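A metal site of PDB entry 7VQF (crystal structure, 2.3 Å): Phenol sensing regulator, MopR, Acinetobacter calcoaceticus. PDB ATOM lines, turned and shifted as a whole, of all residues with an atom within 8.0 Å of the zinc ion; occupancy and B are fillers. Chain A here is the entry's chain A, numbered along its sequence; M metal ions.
Of the 26 residues printed, 4 come within 4 Å of the zinc ion. The nearest printed residue that does not touch the zinc ion is Val 182 (4.1 Å).
The side-chain sulfur (SG) of Cys 189 lies close to the backbone NH (N) of Val 182 (3.3 Å). The side-chain sulfur of Cys 155 lies close to the backbone NH of Ala 140, 3.8 Å away. SG of Cys 155 sits close to OG of Ser 137 (3.0 Å). SG of Cys 181 lies close to N of Ala 154, at 3.4 Å. The side-chain sulfur (SG) of Cys 181 sits close to the backbone NH (N) of Ala 183 (3.4 Å). The backbone carbonyl oxygen (O) of Cys 189 sits at hydrogen-bond distance from the backbone NH (N) of Trp 134 (2.6 Å). The side-chain carboxylate of Asp 186 sits at hydrogen-bond distance from the backbone NH of Cys 181 (3.0 Å).
OE2 of Glu 178 binds the zinc ion, at 1.9 Å. The side-chain sulfur (SG) of Cys 181 binds the zinc ion (2.3 Å). The zinc ion is bound by SG of Cys 155 (2.3 Å). The side-chain sulfur (SG) of Cys 189 binds the zinc ion, at 2.3 Å.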
ATOM      1  N   VAL A 112      21.789  27.818 -22.438  1.00  0.00           N
ATOM      2  CA  VAL A 112      20.968  26.673 -22.043  1.00  0.00           C
ATOM      3  C   VAL A 112      21.836  25.627 -21.352  1.00  0.00           C
ATOM      4  O   VAL A 112      23.031  25.519 -21.632  1.00  0.00           O
ATOM      5  CB  VAL A 112      20.237  26.084 -23.261  1.00  0.00           C
ATOM      6  CG1 VAL A 112      21.223  25.462 -24.243  1.00  0.00           C
ATOM      7  CG2 VAL A 112      19.182  25.072 -22.829  1.00  0.00           C
ATOM      8  N   TRP A 134      16.837  20.271 -22.472  1.00  0.00           N
ATOM      9  CA  TRP A 134      17.299  21.656 -22.396  1.00  0.00           C
ATOM     10  C   TRP A 134      16.681  22.289 -21.162  1.00  0.00           C
ATOM     11  O   TRP A 134      15.465  22.532 -21.110  1.00  0.00           O
ATOM     12  CB  TRP A 134      16.913  22.437 -23.657  1.00  0.00           C
ATOM     13  CG  TRP A 134      17.944  22.408 -24.731  1.00  0.00           C
ATOM     14  CD1 TRP A 134      19.252  22.010 -24.607  1.00  0.00           C
ATOM     15  CD2 TRP A 134      17.768  22.792 -26.093  1.00  0.00           C
ATOM     16  NE1 TRP A 134      19.892  22.133 -25.828  1.00  0.00           N
ATOM     17  CE2 TRP A 134      19.005  22.612 -26.753  1.00  0.00           C
ATOM     18  CE3 TRP A 134      16.680  23.277 -26.829  1.00  0.00           C
ATOM     19  CZ2 TRP A 134      19.180  22.889 -28.097  1.00  0.00           C
ATOM     20  CZ3 TRP A 134      16.858  23.563 -28.173  1.00  0.00           C
ATOM     21  CH2 TRP A 134      18.101  23.361 -28.790  1.00  0.00           C
ATOM     22  N   SER A 137      16.350  27.263 -20.536  1.00  0.00           N
ATOM     23  CA  SER A 137      16.514  27.846 -21.868  1.00  0.00           C
ATOM     24  C   SER A 137      16.280  29.348 -21.820  1.00  0.00           C
ATOM     25  O   SER A 137      15.207  29.805 -21.416  1.00  0.00           O
ATOM     26  CB  SER A 137      15.550  27.189 -22.849  1.00  0.00           C
ATOM     27  OG  SER A 137      15.519  27.903 -24.070  1.00  0.00           O
ATOM     28  N   PHE A 138      17.292  30.122 -22.239  1.00  0.00           N
ATOM     29  CA  PHE A 138      17.115  31.567 -22.338  1.00  0.00           C
ATOM     30  C   PHE A 138      16.055  31.922 -23.362  1.00  0.00           C
ATOM     31  O   PHE A 138      15.281  32.866 -23.163  1.00  0.00           O
ATOM     32  CB  PHE A 138      18.450  32.243 -22.698  1.00  0.00           C
ATOM     33  CG  PHE A 138      18.596  32.550 -24.171  1.00  0.00           C
ATOM     34  CD1 PHE A 138      19.143  31.600 -25.025  1.00  0.00           C
ATOM     35  CD2 PHE A 138      18.178  33.760 -24.706  1.00  0.00           C
ATOM     36  CE1 PHE A 138      19.270  31.861 -26.386  1.00  0.00           C
ATOM     37  CE2 PHE A 138      18.304  34.021 -26.052  1.00  0.00           C
ATOM     38  CZ  PHE A 138      18.850  33.071 -26.893  1.00  0.00           C
ATOM     39  N   GLU A 139      16.014  31.185 -24.473  1.00  0.00           N
ATOM     40  CA  GLU A 139      15.121  31.543 -25.574  1.00  0.00           C
ATOM     41  C   GLU A 139      13.669  31.311 -25.194  1.00  0.00           C
ATOM     42  O   GLU A 139      12.782  32.076 -25.595  1.00  0.00           O
ATOM     43  CB  GLU A 139      15.493  30.755 -26.828  1.00  0.00           C
ATOM     44  CG  GLU A 139      15.109  31.442 -28.116  1.00  0.00           C
ATOM     45  CD  GLU A 139      15.805  30.827 -29.318  1.00  0.00           C
ATOM     46  OE1 GLU A 139      16.529  29.831 -29.137  1.00  0.00           O
ATOM     47  OE2 GLU A 139      15.611  31.338 -30.441  1.00  0.00           O
ATOM     48  N   ALA A 140      13.401  30.243 -24.432  1.00  0.00           N
ATOM     49  CA  ALA A 140      12.039  30.004 -23.969  1.00  0.00           C
ATOM     50  C   ALA A 140      11.582  31.114 -23.039  1.00  0.00           C
ATOM     51  O   ALA A 140      10.440  31.598 -23.162  1.00  0.00           O
ATOM     52  CB  ALA A 140      11.965  28.638 -23.281  1.00  0.00           C
ATOM     53  N   GLU A 141      12.441  31.542 -22.113  1.00  0.00           N
ATOM     54  CA  GLU A 141      12.100  32.659 -21.241  1.00  0.00           C
ATOM     55  C   GLU A 141      11.909  33.939 -22.034  1.00  0.00           C
ATOM     56  O   GLU A 141      10.973  34.701 -21.772  1.00  0.00           O
ATOM     57  CB  GLU A 141      13.195  32.857 -20.188  1.00  0.00           C
ATOM     58  CG  GLU A 141      13.394  31.677 -19.254  1.00  0.00           C
ATOM     59  CD  GLU A 141      14.342  31.993 -18.110  1.00  0.00           C
ATOM     60  OE1 GLU A 141      14.597  33.187 -17.868  1.00  0.00           O
ATOM     61  OE2 GLU A 141      14.827  31.043 -17.467  1.00  0.00           O
ATOM     62  N   HIS A 143      11.048  34.176 -25.193  1.00  0.00           N
ATOM     63  CA  HIS A 143       9.809  34.039 -25.956  1.00  0.00           C
ATOM     64  C   HIS A 143       8.591  34.294 -25.076  1.00  0.00           C
ATOM     65  O   HIS A 143       7.644  34.952 -25.508  1.00  0.00           O
ATOM     66  CB  HIS A 143       9.756  32.641 -26.577  1.00  0.00           C
ATOM     67  CG  HIS A 143       8.581  32.423 -27.471  1.00  0.00           C
ATOM     68  ND1 HIS A 143       8.625  32.604 -28.836  1.00  0.00           N
ATOM     69  CD2 HIS A 143       7.319  32.019 -27.193  1.00  0.00           C
ATOM     70  CE1 HIS A 143       7.451  32.330 -29.354  1.00  0.00           C
ATOM     71  NE2 HIS A 143       6.633  31.971 -28.382  1.00  0.00           N
ATOM     72  N   GLN A 152       3.752  25.968 -30.915  1.00  0.00           N
ATOM     73  CA  GLN A 152       4.914  25.234 -31.392  1.00  0.00           C
ATOM     74  C   GLN A 152       6.136  25.595 -30.553  1.00  0.00           C
ATOM     75  O   GLN A 152       6.180  26.650 -29.924  1.00  0.00           O
ATOM     76  CB  GLN A 152       5.191  25.554 -32.866  1.00  0.00           C
ATOM     77  CG  GLN A 152       4.148  25.004 -33.830  1.00  0.00           C
ATOM     78  CD  GLN A 152       3.909  23.518 -33.653  1.00  0.00           C
ATOM     79  OE1 GLN A 152       2.812  23.093 -33.254  1.00  0.00           O
ATOM     80  NE2 GLN A 152       4.921  22.712 -33.939  1.00  0.00           N
ATOM     81  N   PRO A 153       7.156  24.720 -30.527  1.00  0.00           N
ATOM     82  CA  PRO A 153       8.370  25.042 -29.773  1.00  0.00           C
ATOM     83  C   PRO A 153       9.038  26.299 -30.303  1.00  0.00           C
ATOM     84  O   PRO A 153       8.932  26.627 -31.484  1.00  0.00           O
ATOM     85  CB  PRO A 153       9.244  23.797 -29.966  1.00  0.00           C
ATOM     86  CG  PRO A 153       8.277  22.704 -30.294  1.00  0.00           C
ATOM     87  CD  PRO A 153       7.219  23.370 -31.114  1.00  0.00           C
ATOM     88  N   ALA A 154       9.755  26.980 -29.412  1.00  0.00           N
ATOM     89  CA  ALA A 154      10.219  28.337 -29.684  1.00  0.00           C
ATOM     90  C   ALA A 154      11.723  28.517 -29.665  1.00  0.00           C
ATOM     91  O   ALA A 154      12.197  29.600 -30.034  1.00  0.00           O
ATOM     92  CB  ALA A 154       9.586  29.321 -28.678  1.00  0.00           C
ATOM     93  N   CYS A 155      12.502  27.523 -29.248  1.00  0.00           N
ATOM     94  CA  CYS A 155      13.943  27.689 -29.084  1.00  0.00           C
ATOM     95  C   CYS A 155      14.647  27.492 -30.435  1.00  0.00           C
ATOM     96  O   CYS A 155      15.381  26.530 -30.671  1.00  0.00           O
ATOM     97  CB  CYS A 155      14.467  26.723 -28.020  1.00  0.00           C
ATOM     98  SG  CYS A 155      13.782  27.058 -26.378  1.00  0.00           S
ATOM     99  N   TRP A 156      14.428  28.468 -31.327  1.00  0.00           N
ATOM    100  CA  TRP A 156      14.932  28.363 -32.682  1.00  0.00           C
ATOM    101  C   TRP A 156      16.428  28.620 -32.771  1.00  0.00           C
ATOM    102  O   TRP A 156      17.143  27.910 -33.476  1.00  0.00           O
ATOM    103  CB  TRP A 156      14.179  29.334 -33.601  1.00  0.00           C
ATOM    104  CG  TRP A 156      12.710  29.390 -33.342  1.00  0.00           C
ATOM    105  CD1 TRP A 156      11.873  28.335 -33.098  1.00  0.00           C
ATOM    106  CD2 TRP A 156      11.891  30.569 -33.309  1.00  0.00           C
ATOM    107  NE1 TRP A 156      10.588  28.786 -32.916  1.00  0.00           N
ATOM    108  CE2 TRP A 156      10.572  30.151 -33.027  1.00  0.00           C
ATOM    109  CE3 TRP A 156      12.145  31.936 -33.478  1.00  0.00           C
ATOM    110  CZ2 TRP A 156       9.508  31.048 -32.928  1.00  0.00           C
ATOM    111  CZ3 TRP A 156      11.091  32.819 -33.364  1.00  0.00           C
ATOM    112  CH2 TRP A 156       9.794  32.374 -33.095  1.00  0.00           C
ATOM    113  N   LEU A 158      18.640  28.253 -30.329  1.00  0.00           N
ATOM    114  CA  LEU A 158      19.299  27.116 -29.712  1.00  0.00           C
ATOM    115  C   LEU A 158      19.299  25.914 -30.649  1.00  0.00           C
ATOM    116  O   LEU A 158      20.282  25.167 -30.718  1.00  0.00           O
ATOM    117  CB  LEU A 158      18.610  26.755 -28.393  1.00  0.00           C
ATOM    118  CG  LEU A 158      18.622  27.783 -27.270  1.00  0.00           C
ATOM    119  CD1 LEU A 158      17.971  27.192 -26.019  1.00  0.00           C
ATOM    120  CD2 LEU A 158      20.038  28.258 -26.959  1.00  0.00           C
ATOM    121  N   GLU A 178      12.999  20.055 -31.740  1.00  0.00           N
ATOM    122  CA  GLU A 178      12.621  20.288 -30.351  1.00  0.00           C
ATOM    123  C   GLU A 178      11.269  19.630 -30.106  1.00  0.00           C
ATOM    124  O   GLU A 178      10.225  20.140 -30.535  1.00  0.00           O
ATOM    125  CB  GLU A 178      12.572  21.784 -30.047  1.00  0.00           C
ATOM    126  CG  GLU A 178      12.504  22.100 -28.565  1.00  0.00           C
ATOM    127  CD  GLU A 178      12.562  23.584 -28.262  1.00  0.00           C
ATOM    128  OE1 GLU A 178      12.294  24.397 -29.170  1.00  0.00           O
ATOM    129  OE2 GLU A 178      12.877  23.934 -27.114  1.00  0.00           O
ATOM    130  N   THR A 179      11.269  18.482 -29.422  1.00  0.00           N
ATOM    131  CA  THR A 179      10.022  17.760 -29.164  1.00  0.00           C
ATOM    132  C   THR A 179       9.193  18.428 -28.075  1.00  0.00           C
ATOM    133  O   THR A 179       7.957  18.438 -28.152  1.00  0.00           O
ATOM    134  CB  THR A 179      10.310  16.310 -28.798  1.00  0.00           C
ATOM    135  OG1 THR A 179      11.035  16.252 -27.565  1.00  0.00           O
ATOM    136  CG2 THR A 179      11.120  15.628 -29.888  1.00  0.00           C
ATOM    137  N   HIS A 180       9.849  18.979 -27.060  1.00  0.00           N
ATOM    138  CA  HIS A 180       9.178  19.661 -25.956  1.00  0.00           C
ATOM    139  C   HIS A 180       9.838  21.015 -25.736  1.00  0.00           C
ATOM    140  O   HIS A 180      11.030  21.189 -26.002  1.00  0.00           O
ATOM    141  CB  HIS A 180       9.228  18.825 -24.662  1.00  0.00           C
ATOM    142  CG  HIS A 180       8.648  17.456 -24.807  1.00  0.00           C
ATOM    143  ND1 HIS A 180       9.235  16.483 -25.582  1.00  0.00           N
ATOM    144  CD2 HIS A 180       7.541  16.898 -24.274  1.00  0.00           C
ATOM    145  CE1 HIS A 180       8.517  15.373 -25.522  1.00  0.00           C
ATOM    146  NE2 HIS A 180       7.475  15.606 -24.733  1.00  0.00           N
ATOM    147  N   CYS A 181       9.052  21.969 -25.240  1.00  0.00           N
ATOM    148  CA  CYS A 181       9.549  23.321 -25.028  1.00  0.00           C
ATOM    149  C   CYS A 181       8.797  23.985 -23.886  1.00  0.00           C
ATOM    150  O   CYS A 181       7.574  23.874 -23.791  1.00  0.00           O
ATOM    151  CB  CYS A 181       9.435  24.165 -26.304  1.00  0.00           C
ATOM    152  SG  CYS A 181      10.181  25.808 -26.201  1.00  0.00           S
ATOM    153  N   VAL A 182       9.544  24.688 -23.029  1.00  0.00           N
ATOM    154  CA  VAL A 182       8.934  25.466 -21.951  1.00  0.00           C
ATOM    155  C   VAL A 182       7.916  26.451 -22.515  1.00  0.00           C
ATOM    156  O   VAL A 182       6.839  26.656 -21.947  1.00  0.00           O
ATOM    157  CB  VAL A 182      10.023  26.192 -21.141  1.00  0.00           C
ATOM    158  CG1 VAL A 182       9.406  27.278 -20.255  1.00  0.00           C
ATOM    159  CG2 VAL A 182      10.807  25.212 -20.305  1.00  0.00           C
ATOM    160  N   ALA A 183       8.229  27.070 -23.655  1.00  0.00           N
ATOM    161  CA  ALA A 183       7.320  28.012 -24.285  1.00  0.00           C
ATOM    162  C   ALA A 183       6.053  27.358 -24.814  1.00  0.00           C
ATOM    163  O   ALA A 183       5.132  28.082 -25.223  1.00  0.00           O
ATOM    164  CB  ALA A 183       8.034  28.760 -25.412  1.00  0.00           C
ATOM    165  N   GLN A 184       5.990  26.030 -24.841  1.00  0.00           N
ATOM    166  CA  GLN A 184       4.782  25.304 -25.211  1.00  0.00           C
ATOM    167  C   GLN A 184       3.952  24.893 -24.012  1.00  0.00           C
ATOM    168  O   GLN A 184       2.834  24.399 -24.194  1.00  0.00           O
ATOM    169  CB  GLN A 184       5.135  24.046 -26.010  1.00  0.00           C
ATOM    170  CG  GLN A 184       4.950  24.183 -27.500  1.00  0.00           C
ATOM    171  CD  GLN A 184       5.046  22.845 -28.206  1.00  0.00           C
ATOM    172  OE1 GLN A 184       4.689  22.717 -29.377  1.00  0.00           O
ATOM    173  NE2 GLN A 184       5.536  21.831 -27.491  1.00  0.00           N
ATOM    174  N   ASP A 186       5.369  22.751 -21.640  1.00  0.00           N
ATOM    175  CA  ASP A 186       6.075  21.621 -21.063  1.00  0.00           C
ATOM    176  C   ASP A 186       7.007  22.098 -19.956  1.00  0.00           C
ATOM    177  O   ASP A 186       7.368  23.273 -19.863  1.00  0.00           O
ATOM    178  CB  ASP A 186       6.858  20.873 -22.147  1.00  0.00           C
ATOM    179  CG  ASP A 186       5.996  20.491 -23.329  1.00  0.00           C
ATOM    180  OD1 ASP A 186       4.883  19.959 -23.107  1.00  0.00           O
ATOM    181  OD2 ASP A 186       6.407  20.725 -24.484  1.00  0.00           O
ATOM    182  N   HIS A 188      10.219  21.343 -19.239  1.00  0.00           N
ATOM    183  CA  HIS A 188      11.482  21.803 -19.786  1.00  0.00           C
ATOM    184  C   HIS A 188      11.508  21.468 -21.278  1.00  0.00           C
ATOM    185  O   HIS A 188      10.570  20.871 -21.819  1.00  0.00           O
ATOM    186  CB  HIS A 188      12.681  21.199 -19.044  1.00  0.00           C
ATOM    187  CG  HIS A 188      12.698  19.700 -19.039  1.00  0.00           C
ATOM    188  ND1 HIS A 188      12.965  18.953 -20.163  1.00  0.00           N
ATOM    189  CD2 HIS A 188      12.517  18.812 -18.033  1.00  0.00           C
ATOM    190  CE1 HIS A 188      12.937  17.672 -19.856  1.00  0.00           C
ATOM    191  NE2 HIS A 188      12.664  17.551 -18.573  1.00  0.00           N
ATOM    192  N   CYS A 189      12.589  21.869 -21.940  1.00  0.00           N
ATOM    193  CA  CYS A 189      12.742  21.620 -23.369  1.00  0.00           C
ATOM    194  C   CYS A 189      13.513  20.322 -23.595  1.00  0.00           C
ATOM    195  O   CYS A 189      14.277  19.861 -22.748  1.00  0.00           O
ATOM    196  CB  CYS A 189      13.456  22.780 -24.044  1.00  0.00           C
ATOM    197  SG  CYS A 189      12.739  24.416 -23.746  1.00  0.00           S
ATOM    198  N   ARG A 190      13.288  19.725 -24.765  1.00  0.00           N
ATOM    199  CA  ARG A 190      13.914  18.463 -25.126  1.00  0.00           C
ATOM    200  C   ARG A 190      14.076  18.422 -26.640  1.00  0.00           C
ATOM    201  O   ARG A 190      13.209  18.903 -27.379  1.00  0.00           O
ATOM    202  CB  ARG A 190      13.075  17.270 -24.648  1.00  0.00           C
ATOM    203  CG  ARG A 190      13.710  15.910 -24.895  1.00  0.00           C
ATOM    204  CD  ARG A 190      12.634  14.870 -25.087  1.00  0.00           C
ATOM    205  NE  ARG A 190      13.163  13.574 -25.495  1.00  0.00           N
ATOM    206  CZ  ARG A 190      12.599  12.806 -26.420  1.00  0.00           C
ATOM    207  NH1 ARG A 190      11.533  13.200 -27.091  1.00  0.00           N
ATOM    208  NH2 ARG A 190      13.130  11.613 -26.680  1.00  0.00           N
ATOM    209  N   ILE A 191      15.196  17.868 -27.099  1.00  0.00           N
ATOM    210  CA  ILE A 191      15.514  17.799 -28.513  1.00  0.00           C
ATOM    211  C   ILE A 191      15.946  16.386 -28.869  1.00  0.00           C
ATOM    212  O   ILE A 191      16.366  15.601 -28.017  1.00  0.00           O
ATOM    213  CB  ILE A 191      16.615  18.797 -28.921  1.00  0.00           C
ATOM    214  CG1 ILE A 191      17.957  18.371 -28.321  1.00  0.00           C
ATOM    215  CG2 ILE A 191      16.237  20.202 -28.491  1.00  0.00           C
ATOM    216  CD1 ILE A 191      19.060  19.387 -28.509  1.00  0.00           C
HETATM  217 ZN    ZN M   1      12.391  25.300 -25.848  1.00  0.00          ZN
